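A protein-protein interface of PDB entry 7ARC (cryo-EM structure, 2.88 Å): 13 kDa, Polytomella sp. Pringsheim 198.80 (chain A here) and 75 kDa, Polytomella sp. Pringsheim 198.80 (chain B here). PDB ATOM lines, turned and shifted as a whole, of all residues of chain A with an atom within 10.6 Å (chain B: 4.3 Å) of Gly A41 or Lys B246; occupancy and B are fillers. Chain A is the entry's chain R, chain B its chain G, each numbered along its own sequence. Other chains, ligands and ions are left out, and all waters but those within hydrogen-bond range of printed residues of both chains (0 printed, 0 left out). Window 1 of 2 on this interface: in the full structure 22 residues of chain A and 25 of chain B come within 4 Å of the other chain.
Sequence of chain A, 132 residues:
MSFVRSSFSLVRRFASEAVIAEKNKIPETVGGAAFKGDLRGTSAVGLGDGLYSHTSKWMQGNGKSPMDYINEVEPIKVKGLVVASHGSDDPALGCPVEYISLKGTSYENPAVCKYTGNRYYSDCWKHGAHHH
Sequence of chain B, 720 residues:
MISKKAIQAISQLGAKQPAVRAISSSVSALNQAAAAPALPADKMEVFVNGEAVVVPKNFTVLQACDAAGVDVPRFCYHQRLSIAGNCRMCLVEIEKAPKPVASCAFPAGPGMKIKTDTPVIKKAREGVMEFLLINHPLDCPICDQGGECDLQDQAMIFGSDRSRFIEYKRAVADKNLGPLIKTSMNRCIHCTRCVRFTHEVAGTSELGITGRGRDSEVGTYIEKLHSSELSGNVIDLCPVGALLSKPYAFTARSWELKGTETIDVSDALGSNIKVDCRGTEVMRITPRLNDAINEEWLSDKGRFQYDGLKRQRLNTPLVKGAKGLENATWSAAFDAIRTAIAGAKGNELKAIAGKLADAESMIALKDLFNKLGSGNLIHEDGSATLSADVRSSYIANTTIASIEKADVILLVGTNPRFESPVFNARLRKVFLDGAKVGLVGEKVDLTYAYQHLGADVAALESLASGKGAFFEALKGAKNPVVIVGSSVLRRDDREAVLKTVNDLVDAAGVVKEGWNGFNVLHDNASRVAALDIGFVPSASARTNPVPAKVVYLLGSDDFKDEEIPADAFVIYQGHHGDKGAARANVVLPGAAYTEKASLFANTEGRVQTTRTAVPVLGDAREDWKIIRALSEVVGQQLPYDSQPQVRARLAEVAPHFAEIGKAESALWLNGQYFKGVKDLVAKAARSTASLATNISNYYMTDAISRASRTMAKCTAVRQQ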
ATOM      1  N   ILE A  26      17.016  -1.904  -0.004  1.00  0.00           N
ATOM      2  CA  ILE A  26      17.568  -2.963   0.842  1.00  0.00           C
ATOM      3  C   ILE A  26      16.467  -3.980   1.126  1.00  0.00           C
ATOM      4  O   ILE A  26      15.356  -3.585   1.513  1.00  0.00           O
ATOM      5  CB  ILE A  26      18.124  -2.382   2.137  1.00  0.00           C
ATOM      6  CG1 ILE A  26      19.020  -1.175   1.847  1.00  0.00           C
ATOM      7  CG2 ILE A  26      18.892  -3.441   2.911  1.00  0.00           C
ATOM      8  CD1 ILE A  26      20.219  -1.494   0.990  1.00  0.00           C
ATOM      9  N   PRO A  27      16.717  -5.273   0.923  1.00  0.00           N
ATOM     10  CA  PRO A  27      15.724  -6.285   1.305  1.00  0.00           C
ATOM     11  C   PRO A  27      15.389  -6.195   2.786  1.00  0.00           C
ATOM     12  O   PRO A  27      16.274  -6.218   3.643  1.00  0.00           O
ATOM     13  CB  PRO A  27      16.414  -7.614   0.970  1.00  0.00           C
ATOM     14  CG  PRO A  27      17.642  -7.275   0.185  1.00  0.00           C
ATOM     15  CD  PRO A  27      17.737  -5.801   0.004  1.00  0.00           C
ATOM     16  N   GLU A  28      14.096  -6.103   3.082  1.00  0.00           N
ATOM     17  CA  GLU A  28      13.629  -5.898   4.442  1.00  0.00           C
ATOM     18  C   GLU A  28      12.538  -6.910   4.759  1.00  0.00           C
ATOM     19  O   GLU A  28      11.942  -7.516   3.866  1.00  0.00           O
ATOM     20  CB  GLU A  28      13.079  -4.475   4.633  1.00  0.00           C
ATOM     21  CG  GLU A  28      14.110  -3.362   4.506  1.00  0.00           C
ATOM     22  CD  GLU A  28      15.141  -3.379   5.611  1.00  0.00           C
ATOM     23  OE1 GLU A  28      14.795  -3.785   6.739  1.00  0.00           O
ATOM     24  OE2 GLU A  28      16.297  -2.984   5.353  1.00  0.00           O
ATOM     25  N   THR A  29      12.282  -7.077   6.051  1.00  0.00           N
ATOM     26  CA  THR A  29      11.274  -8.001   6.552  1.00  0.00           C
ATOM     27  C   THR A  29      10.125  -7.207   7.160  1.00  0.00           C
ATOM     28  O   THR A  29      10.353  -6.239   7.893  1.00  0.00           O
ATOM     29  CB  THR A  29      11.881  -8.990   7.555  1.00  0.00           C
ATOM     30  OG1 THR A  29      10.868  -9.881   8.037  1.00  0.00           O
ATOM     31  CG2 THR A  29      12.545  -8.273   8.709  1.00  0.00           C
ATOM     32  N   VAL A  30       8.894  -7.601   6.827  1.00  0.00           N
ATOM     33  CA  VAL A  30       7.714  -6.933   7.374  1.00  0.00           C
ATOM     34  C   VAL A  30       7.687  -7.023   8.894  1.00  0.00           C
ATOM     35  O   VAL A  30       7.388  -6.038   9.580  1.00  0.00           O
ATOM     36  CB  VAL A  30       6.434  -7.520   6.751  1.00  0.00           C
ATOM     37  CG1 VAL A  30       5.205  -6.905   7.391  1.00  0.00           C
ATOM     38  CG2 VAL A  30       6.426  -7.287   5.252  1.00  0.00           C
ATOM     39  N   GLY A  31       7.998  -8.186   9.446  1.00  0.00           N
ATOM     40  CA  GLY A  31       8.137  -8.331  10.875  1.00  0.00           C
ATOM     41  C   GLY A  31       7.091  -9.173  11.590  1.00  0.00           C
ATOM     42  O   GLY A  31       6.958  -9.044  12.813  1.00  0.00           O
ATOM     43  N   ALA A  33       6.974 -12.619  11.936  1.00  0.00           N
ATOM     44  CA  ALA A  33       7.803 -13.516  12.734  1.00  0.00           C
ATOM     45  C   ALA A  33       9.213 -12.977  12.933  1.00  0.00           C
ATOM     46  O   ALA A  33      10.082 -13.700  13.431  1.00  0.00           O
ATOM     47  CB  ALA A  33       7.859 -14.901  12.086  1.00  0.00           C
ATOM     48  N   ALA A  34       9.453 -11.728  12.556  1.00  0.00           N
ATOM     49  CA  ALA A  34      10.763 -11.096  12.644  1.00  0.00           C
ATOM     50  C   ALA A  34      10.541  -9.686  13.178  1.00  0.00           C
ATOM     51  O   ALA A  34       9.488  -9.370  13.742  1.00  0.00           O
ATOM     52  CB  ALA A  34      11.476 -11.130  11.284  1.00  0.00           C
ATOM     53  N   PHE A  35      11.538  -8.825  13.029  1.00  0.00           N
ATOM     54  CA  PHE A  35      11.443  -7.457  13.508  1.00  0.00           C
ATOM     55  C   PHE A  35      11.201  -6.525  12.327  1.00  0.00           C
ATOM     56  O   PHE A  35      11.451  -6.873  11.173  1.00  0.00           O
ATOM     57  CB  PHE A  35      12.706  -7.051  14.267  1.00  0.00           C
ATOM     58  CG  PHE A  35      12.845  -7.719  15.601  1.00  0.00           C
ATOM     59  CD1 PHE A  35      11.966  -7.432  16.630  1.00  0.00           C
ATOM     60  CD2 PHE A  35      13.848  -8.646  15.822  1.00  0.00           C
ATOM     61  CE1 PHE A  35      12.090  -8.050  17.858  1.00  0.00           C
ATOM     62  CE2 PHE A  35      13.975  -9.268  17.044  1.00  0.00           C
ATOM     63  CZ  PHE A  35      13.094  -8.970  18.064  1.00  0.00           C
ATOM     64  N   LYS A  36      10.688  -5.334  12.631  1.00  0.00           N
ATOM     65  CA  LYS A  36      10.213  -4.440  11.579  1.00  0.00           C
ATOM     66  C   LYS A  36      11.333  -4.017  10.634  1.00  0.00           C
ATOM     67  O   LYS A  36      11.109  -3.875   9.426  1.00  0.00           O
ATOM     68  CB  LYS A  36       9.550  -3.216  12.208  1.00  0.00           C
ATOM     69  CG  LYS A  36       8.963  -2.235  11.212  1.00  0.00           C
ATOM     70  CD  LYS A  36       7.855  -2.893  10.408  1.00  0.00           C
ATOM     71  CE  LYS A  36       6.669  -3.248  11.294  1.00  0.00           C
ATOM     72  NZ  LYS A  36       5.961  -2.044  11.809  1.00  0.00           N
ATOM     73  N   GLY A  37      12.541  -3.810  11.152  1.00  0.00           N
ATOM     74  CA  GLY A  37      13.593  -3.247  10.326  1.00  0.00           C
ATOM     75  C   GLY A  37      14.794  -4.126  10.038  1.00  0.00           C
ATOM     76  O   GLY A  37      15.857  -3.612   9.680  1.00  0.00           O
ATOM     77  N   ASP A  38      14.653  -5.440  10.178  1.00  0.00           N
ATOM     78  CA  ASP A  38      15.788  -6.327   9.980  1.00  0.00           C
ATOM     79  C   ASP A  38      16.070  -6.562   8.500  1.00  0.00           C
ATOM     80  O   ASP A  38      15.221  -6.350   7.631  1.00  0.00           O
ATOM     81  CB  ASP A  38      15.562  -7.676  10.659  1.00  0.00           C
ATOM     82  CG  ASP A  38      15.576  -7.581  12.162  1.00  0.00           C
ATOM     83  OD1 ASP A  38      16.260  -6.685  12.699  1.00  0.00           O
ATOM     84  OD2 ASP A  38      14.944  -8.442  12.806  1.00  0.00           O
ATOM     85  N   LEU A  39      17.291  -7.016   8.225  1.00  0.00           N
ATOM     86  CA  LEU A  39      17.595  -7.615   6.935  1.00  0.00           C
ATOM     87  C   LEU A  39      16.813  -8.902   6.732  1.00  0.00           C
ATOM     88  O   LEU A  39      16.477  -9.615   7.680  1.00  0.00           O
ATOM     89  CB  LEU A  39      19.088  -7.916   6.793  1.00  0.00           C
ATOM     90  CG  LEU A  39      20.082  -6.771   6.722  1.00  0.00           C
ATOM     91  CD1 LEU A  39      21.492  -7.315   6.738  1.00  0.00           C
ATOM     92  CD2 LEU A  39      19.824  -6.055   5.416  1.00  0.00           C
ATOM     93  N   ARG A  40      16.519  -9.182   5.473  1.00  0.00           N
ATOM     94  CA  ARG A  40      15.901 -10.430   5.065  1.00  0.00           C
ATOM     95  C   ARG A  40      16.973 -11.307   4.436  1.00  0.00           C
ATOM     96  O   ARG A  40      17.704 -10.858   3.547  1.00  0.00           O
ATOM     97  CB  ARG A  40      14.778 -10.165   4.066  1.00  0.00           C
ATOM     98  CG  ARG A  40      13.705 -11.217   4.019  1.00  0.00           C
ATOM     99  CD  ARG A  40      12.652 -10.826   3.010  1.00  0.00           C
ATOM    100  NE  ARG A  40      12.862 -11.515   1.743  1.00  0.00           N
ATOM    101  CZ  ARG A  40      12.950 -10.908   0.569  1.00  0.00           C
ATOM    102  NH1 ARG A  40      12.824  -9.596   0.460  1.00  0.00           N
ATOM    103  NH2 ARG A  40      13.169 -11.634  -0.522  1.00  0.00           N
ATOM    104  N   GLY A  41      17.080 -12.545   4.910  1.00  0.00           N
ATOM    105  CA  GLY A  41      17.985 -13.485   4.284  1.00  0.00           C
ATOM    106  C   GLY A  41      17.555 -13.763   2.861  1.00  0.00           C
ATOM    107  O   GLY A  41      16.430 -14.210   2.629  1.00  0.00           O
ATOM    108  N   THR A  42      18.433 -13.501   1.899  1.00  0.00           N
ATOM    109  CA  THR A  42      18.081 -13.610   0.492  1.00  0.00           C
ATOM    110  C   THR A  42      19.151 -14.381  -0.261  1.00  0.00           C
ATOM    111  O   THR A  42      20.349 -14.187  -0.036  1.00  0.00           O
ATOM    112  CB  THR A  42      17.897 -12.232  -0.155  1.00  0.00           C
ATOM    113  OG1 THR A  42      18.944 -11.354   0.278  1.00  0.00           O
ATOM    114  CG2 THR A  42      16.553 -11.639   0.226  1.00  0.00           C
ATOM    115  N   SER A  43      18.706 -15.260  -1.152  1.00  0.00           N
ATOM    116  CA  SER A  43      19.579 -15.864  -2.140  1.00  0.00           C
ATOM    117  C   SER A  43      19.551 -15.004  -3.400  1.00  0.00           C
ATOM    118  O   SER A  43      18.831 -14.008  -3.485  1.00  0.00           O
ATOM    119  CB  SER A  43      19.158 -17.305  -2.425  1.00  0.00           C
ATOM    120  OG  SER A  43      17.753 -17.410  -2.572  1.00  0.00           O
ATOM    121  N   ALA A  44      20.336 -15.390  -4.397  1.00  0.00           N
ATOM    122  CA  ALA A  44      20.436 -14.618  -5.625  1.00  0.00           C
ATOM    123  C   ALA A  44      19.458 -15.081  -6.695  1.00  0.00           C
ATOM    124  O   ALA A  44      19.567 -14.648  -7.845  1.00  0.00           O
ATOM    125  CB  ALA A  44      21.866 -14.673  -6.163  1.00  0.00           C
ATOM    126  N   VAL A  45      18.510 -15.953  -6.344  1.00  0.00           N
ATOM    127  CA  VAL A  45      17.494 -16.369  -7.300  1.00  0.00           C
ATOM    128  C   VAL A  45      16.651 -15.176  -7.720  1.00  0.00           C
ATOM    129  O   VAL A  45      16.269 -14.335  -6.896  1.00  0.00           O
ATOM    130  CB  VAL A  45      16.622 -17.474  -6.685  1.00  0.00           C
ATOM    131  CG1 VAL A  45      15.733 -18.106  -7.742  1.00  0.00           C
ATOM    132  CG2 VAL A  45      17.500 -18.506  -6.011  1.00  0.00           C
ATOM    133  N   TYR A  52      12.171  -9.404  -7.066  1.00  0.00           N
ATOM    134  CA  TYR A  52      12.728  -9.092  -5.758  1.00  0.00           C
ATOM    135  C   TYR A  52      11.811  -9.446  -4.597  1.00  0.00           C
ATOM    136  O   TYR A  52      12.160  -9.150  -3.450  1.00  0.00           O
ATOM    137  CB  TYR A  52      13.112  -7.607  -5.661  1.00  0.00           C
ATOM    138  CG  TYR A  52      14.063  -7.154  -6.738  1.00  0.00           C
ATOM    139  CD1 TYR A  52      15.434  -7.278  -6.567  1.00  0.00           C
ATOM    140  CD2 TYR A  52      13.598  -6.589  -7.915  1.00  0.00           C
ATOM    141  CE1 TYR A  52      16.313  -6.865  -7.540  1.00  0.00           C
ATOM    142  CE2 TYR A  52      14.474  -6.171  -8.896  1.00  0.00           C
ATOM    143  CZ  TYR A  52      15.831  -6.313  -8.702  1.00  0.00           C
ATOM    144  OH  TYR A  52      16.713  -5.904  -9.673  1.00  0.00           O
ATOM    145  N   SER A  53      10.665 -10.062  -4.850  1.00  0.00           N
ATOM    146  CA  SER A  53       9.770 -10.499  -3.793  1.00  0.00           C
ATOM    147  C   SER A  53       9.822 -12.015  -3.685  1.00  0.00           C
ATOM    148  O   SER A  53      10.061 -12.714  -4.671  1.00  0.00           O
ATOM    149  CB  SER A  53       8.333 -10.043  -4.060  1.00  0.00           C
ATOM    150  OG  SER A  53       7.457 -10.498  -3.046  1.00  0.00           O
ATOM    151  N   HIS A  54       9.602 -12.515  -2.469  1.00  0.00           N
ATOM    152  CA  HIS A  54       9.661 -13.953  -2.238  1.00  0.00           C
ATOM    153  C   HIS A  54       8.614 -14.688  -3.063  1.00  0.00           C
ATOM    154  O   HIS A  54       8.916 -15.691  -3.719  1.00  0.00           O
ATOM    155  CB  HIS A  54       9.480 -14.248  -0.751  1.00  0.00           C
ATOM    156  CG  HIS A  54       9.862 -15.640  -0.362  1.00  0.00           C
ATOM    157  ND1 HIS A  54       9.004 -16.708  -0.492  1.00  0.00           N
ATOM    158  CD2 HIS A  54      11.010 -16.140   0.152  1.00  0.00           C
ATOM    159  CE1 HIS A  54       9.605 -17.806  -0.073  1.00  0.00           C
ATOM    160  NE2 HIS A  54      10.824 -17.489   0.322  1.00  0.00           N
ATOM    161  N   LYS A  57       9.047 -14.853  -7.005  1.00  0.00           N
ATOM    162  CA  LYS A  57      10.072 -15.742  -7.541  1.00  0.00           C
ATOM    163  C   LYS A  57       9.487 -17.088  -7.942  1.00  0.00           C
ATOM    164  O   LYS A  57       9.929 -17.698  -8.922  1.00  0.00           O
ATOM    165  CB  LYS A  57      11.184 -15.928  -6.512  1.00  0.00           C
ATOM    166  CG  LYS A  57      11.984 -14.672  -6.257  1.00  0.00           C
ATOM    167  CD  LYS A  57      13.091 -14.898  -5.254  1.00  0.00           C
ATOM    168  CE  LYS A  57      13.848 -13.611  -5.009  1.00  0.00           C
ATOM    169  NZ  LYS A  57      14.942 -13.778  -4.020  1.00  0.00           N
ATOM    170  N   ASN B 176      16.505  -8.149  19.167  1.00  0.00           N
ATOM    171  CA  ASN B 176      17.378  -7.732  18.078  1.00  0.00           C
ATOM    172  C   ASN B 176      18.779  -7.426  18.595  1.00  0.00           C
ATOM    173  O   ASN B 176      18.945  -6.657  19.546  1.00  0.00           O
ATOM    174  CB  ASN B 176      16.791  -6.504  17.386  1.00  0.00           C
ATOM    175  CG  ASN B 176      17.108  -6.460  15.906  1.00  0.00           C
ATOM    176  OD1 ASN B 176      17.569  -7.444  15.329  1.00  0.00           O
ATOM    177  ND2 ASN B 176      16.859  -5.316  15.283  1.00  0.00           N
ATOM    178  N   GLY B 178      21.088  -6.556  16.075  1.00  0.00           N
ATOM    179  CA  GLY B 178      21.639  -5.778  14.995  1.00  0.00           C
ATOM    180  C   GLY B 178      21.297  -6.341  13.634  1.00  0.00           C
ATOM    181  O   GLY B 178      20.559  -7.321  13.504  1.00  0.00           O
ATOM    182  N   PRO B 179      21.836  -5.718  12.585  1.00  0.00           N
ATOM    183  CA  PRO B 179      21.510  -6.163  11.224  1.00  0.00           C
ATOM    184  C   PRO B 179      22.128  -7.499  10.849  1.00  0.00           C
ATOM    185  O   PRO B 179      21.630  -8.143   9.920  1.00  0.00           O
ATOM    186  CB  PRO B 179      22.057  -5.031  10.346  1.00  0.00           C
ATOM    187  CG  PRO B 179      23.145  -4.428  11.159  1.00  0.00           C
ATOM    188  CD  PRO B 179      22.689  -4.519  12.586  1.00  0.00           C
ATOM    189  N   LEU B 180      23.195  -7.936  11.519  1.00  0.00           N
ATOM    190  CA  LEU B 180      23.926  -9.111  11.064  1.00  0.00           C
ATOM    191  C   LEU B 180      23.673 -10.366  11.884  1.00  0.00           C
ATOM    192  O   LEU B 180      24.001 -11.460  11.415  1.00  0.00           O
ATOM    193  CB  LEU B 180      25.433  -8.835  11.071  1.00  0.00           C
ATOM    194  CG  LEU B 180      25.919  -7.611  10.307  1.00  0.00           C
ATOM    195  CD1 LEU B 180      27.332  -7.256  10.717  1.00  0.00           C
ATOM    196  CD2 LEU B 180      25.858  -7.899   8.840  1.00  0.00           C
ATOM    197  N   ILE B 181      23.108 -10.253  13.080  1.00  0.00           N
ATOM    198  CA  ILE B 181      22.971 -11.393  13.980  1.00  0.00           C
ATOM    199  C   ILE B 181      21.492 -11.675  14.176  1.00  0.00           C
ATOM    200  O   ILE B 181      20.734 -10.791  14.590  1.00  0.00           O
ATOM    201  CB  ILE B 181      23.669 -11.158  15.327  1.00  0.00           C
ATOM    202  CG1 ILE B 181      25.137 -10.794  15.108  1.00  0.00           C
ATOM    203  CG2 ILE B 181      23.562 -12.391  16.200  1.00  0.00           C
ATOM    204  CD1 ILE B 181      25.689  -9.862  16.150  1.00  0.00           C
ATOM    205  N   LYS B 182      21.087 -12.905  13.888  1.00  0.00           N
ATOM    206  CA  LYS B 182      19.749 -13.380  14.187  1.00  0.00           C
ATOM    207  C   LYS B 182      19.792 -14.192  15.473  1.00  0.00           C
ATOM    208  O   LYS B 182      20.754 -14.919  15.727  1.00  0.00           O
ATOM    209  CB  LYS B 182      19.211 -14.222  13.031  1.00  0.00           C
ATOM    210  CG  LYS B 182      17.804 -14.738  13.207  1.00  0.00           C
ATOM    211  CD  LYS B 182      17.359 -15.439  11.944  1.00  0.00           C
ATOM    212  CE  LYS B 182      18.064 -16.773  11.803  1.00  0.00           C
ATOM    213  NZ  LYS B 182      17.578 -17.549  10.637  1.00  0.00           N
ATOM    214  N   LEU B 244      22.823 -16.722  14.884  1.00  0.00           N
ATOM    215  CA  LEU B 244      22.934 -17.140  13.497  1.00  0.00           C
ATOM    216  C   LEU B 244      23.093 -15.918  12.606  1.00  0.00           C
ATOM    217  O   LEU B 244      22.818 -14.788  13.011  1.00  0.00           O
ATOM    218  CB  LEU B 244      21.708 -17.955  13.071  1.00  0.00           C
ATOM    219  CG  LEU B 244      21.807 -19.468  13.267  1.00  0.00           C
ATOM    220  CD1 LEU B 244      20.457 -20.113  13.053  1.00  0.00           C
ATOM    221  CD2 LEU B 244      22.846 -20.077  12.345  1.00  0.00           C
ATOM    222  N   SER B 245      23.539 -16.162  11.378  1.00  0.00           N
ATOM    223  CA  SER B 245      23.801 -15.084  10.436  1.00  0.00           C
ATOM    224  C   SER B 245      22.501 -14.716   9.739  1.00  0.00           C
ATOM    225  O   SER B 245      21.914 -15.537   9.029  1.00  0.00           O
ATOM    226  CB  SER B 245      24.859 -15.508   9.423  1.00  0.00           C
ATOM    227  OG  SER B 245      24.869 -14.642   8.307  1.00  0.00           O
ATOM    228  N   LYS B 246      22.049 -13.490   9.948  1.00  0.00           N
ATOM    229  CA  LYS B 246      20.827 -12.983   9.341  1.00  0.00           C
ATOM    230  C   LYS B 246      20.922 -12.864   7.819  1.00  0.00           C
ATOM    231  O   LYS B 246      19.960 -13.217   7.128  1.00  0.00           O
ATOM    232  CB  LYS B 246      20.455 -11.652   9.988  1.00  0.00           C
ATOM    233  CG  LYS B 246      19.134 -11.078   9.557  1.00  0.00           C
ATOM    234  CD  LYS B 246      18.944  -9.751  10.238  1.00  0.00           C
ATOM    235  CE  LYS B 246      18.635  -9.965  11.704  1.00  0.00           C
ATOM    236  NZ  LYS B 246      18.335  -8.697  12.407  1.00  0.00           N
ATOM    237  N   PRO B 247      22.022 -12.351   7.247  1.00  0.00           N
ATOM    238  CA  PRO B 247      22.130 -12.377   5.777  1.00  0.00           C
ATOM    239  C   PRO B 247      22.061 -13.777   5.194  1.00  0.00           C
ATOM    240  O   PRO B 247      21.449 -13.980   4.138  1.00  0.00           O
ATOM    241  CB  PRO B 247      23.493 -11.723   5.526  1.00  0.00           C
ATOM    242  CG  PRO B 247      23.660 -10.805   6.663  1.00  0.00           C
ATOM    243  CD  PRO B 247      23.112 -11.554   7.838  1.00  0.00           C
ATOM    244  N   TYR B 248      22.682 -14.750   5.855  1.00  0.00           N
ATOM    245  CA  TYR B 248      22.666 -16.144   5.420  1.00  0.00           C
ATOM    246  C   TYR B 248      21.622 -16.904   6.235  1.00  0.00           C
ATOM    247  O   TYR B 248      21.927 -17.719   7.104  1.00  0.00           O
ATOM    248  CB  TYR B 248      24.057 -16.757   5.567  1.00  0.00           C
ATOM    249  CG  TYR B 248      24.161 -18.219   5.188  1.00  0.00           C
ATOM    250  CD1 TYR B 248      24.125 -18.616   3.861  1.00  0.00           C
ATOM    251  CD2 TYR B 248      24.302 -19.200   6.158  1.00  0.00           C
ATOM    252  CE1 TYR B 248      24.223 -19.948   3.511  1.00  0.00           C
ATOM    253  CE2 TYR B 248      24.395 -20.533   5.819  1.00  0.00           C
ATOM    254  CZ  TYR B 248      24.358 -20.900   4.495  1.00  0.00           C
ATOM    255  OH  TYR B 248      24.455 -22.227   4.153  1.00  0.00           O
ATOM    256  N   ALA B 249      20.361 -16.596   5.958  1.00  0.00           N
ATOM    257  CA  ALA B 249      19.241 -17.137   6.719  1.00  0.00           C
ATOM    258  C   ALA B 249      18.339 -17.929   5.787  1.00  0.00           C
ATOM    259  O   ALA B 249      17.810 -17.380   4.815  1.00  0.00           O
ATOM    260  CB  ALA B 249      18.454 -16.024   7.409  1.00  0.00           C
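The side-chain amino group of Lys B246 is in salt-bridge range of the side-chain carboxylate of Asp A38 (2.9 Å).
OD1 of Asp A38 is in hydrogen-bond range of ND2 of Asn B176, at 3.0 Å.
OD1 of Asn B176 is in hydrogen-bond range of NZ of Lys B246 (3.3 Å).
The backbone carbonyl oxygen (O) of Asp A38 sits at hydrogen-bond distance from the backbone NH (N) of Thr A29 (3.4 Å).
The backbone carbonyl oxygen of Leu B180 sits at hydrogen-bond distance from the backbone NH of Lys B246, 3.2 Å away.
N of Phe A35 lies close to OD2 of Asp A38 (3.4 Å).
O of Gly B178 sits at hydrogen-bond distance from NZ of Lys B246 (2.8 Å).
The backbone carbonyl oxygen (O) of Asp A38 sits close to the side-chain carboxylate (OE1) of Glu A28 (2.7 Å).
CE2 of Phe A35 touches N of Asn B176, 3.5 Å away.
Leu A39 touches Pro B179.
Leu A39 touches Lys B246 (O to CD, 3.6 Å).
Gly A41 touches Lys B246.
CA of Gly A41 touches O of Pro B247, at 3.5 Å.
CA of Gly A41 touches O of Ala B249, 3.9 Å away.
Pro B247 touches Thr A42.
Gly A31 touches none of the printed residues of chain B.
Of the printed residues of chain B, Phe A35 touches Asn B176.
Of the printed residues of chain B, Asp A38 touches Asn B176 and Lys B246.
Gly A41 touches just these residues of chain B: Lys B246, Pro B247 and Ala B249.
Of the printed residues of chain B, Thr A42 touches Pro B247 (3.8 Å).
Of the printed residues of chain A, Asn B176 touches Phe A35 and Asp A38.
No residue of chain A comes within 4 Å of Gly B178.
Printed residues of chain A within 4 Å of Pro B179: Leu A39.
Leu B180 touches none of the printed residues of chain A.
No residue of chain A comes within 4 Å of Ser B245.
Lys B246 touches just these residues of chain A: Asp A38 (2.9 Å), Leu A39 (3.6 Å) and Gly A41 (3.5 Å).
Of the printed residues of chain A, Pro B247 touches Gly A41 (3.5 Å) and Thr A42 (3.8 Å).
Ala B249 touches one residue of chain A.
Along chain A the printed residues that touch a printed residue of chain B span positions 35 to 42.
Of the 12 printed residues of chain B, 5 touch a printed residue of chain A.
Among the printed residues, 9 pairs touch across the chains.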
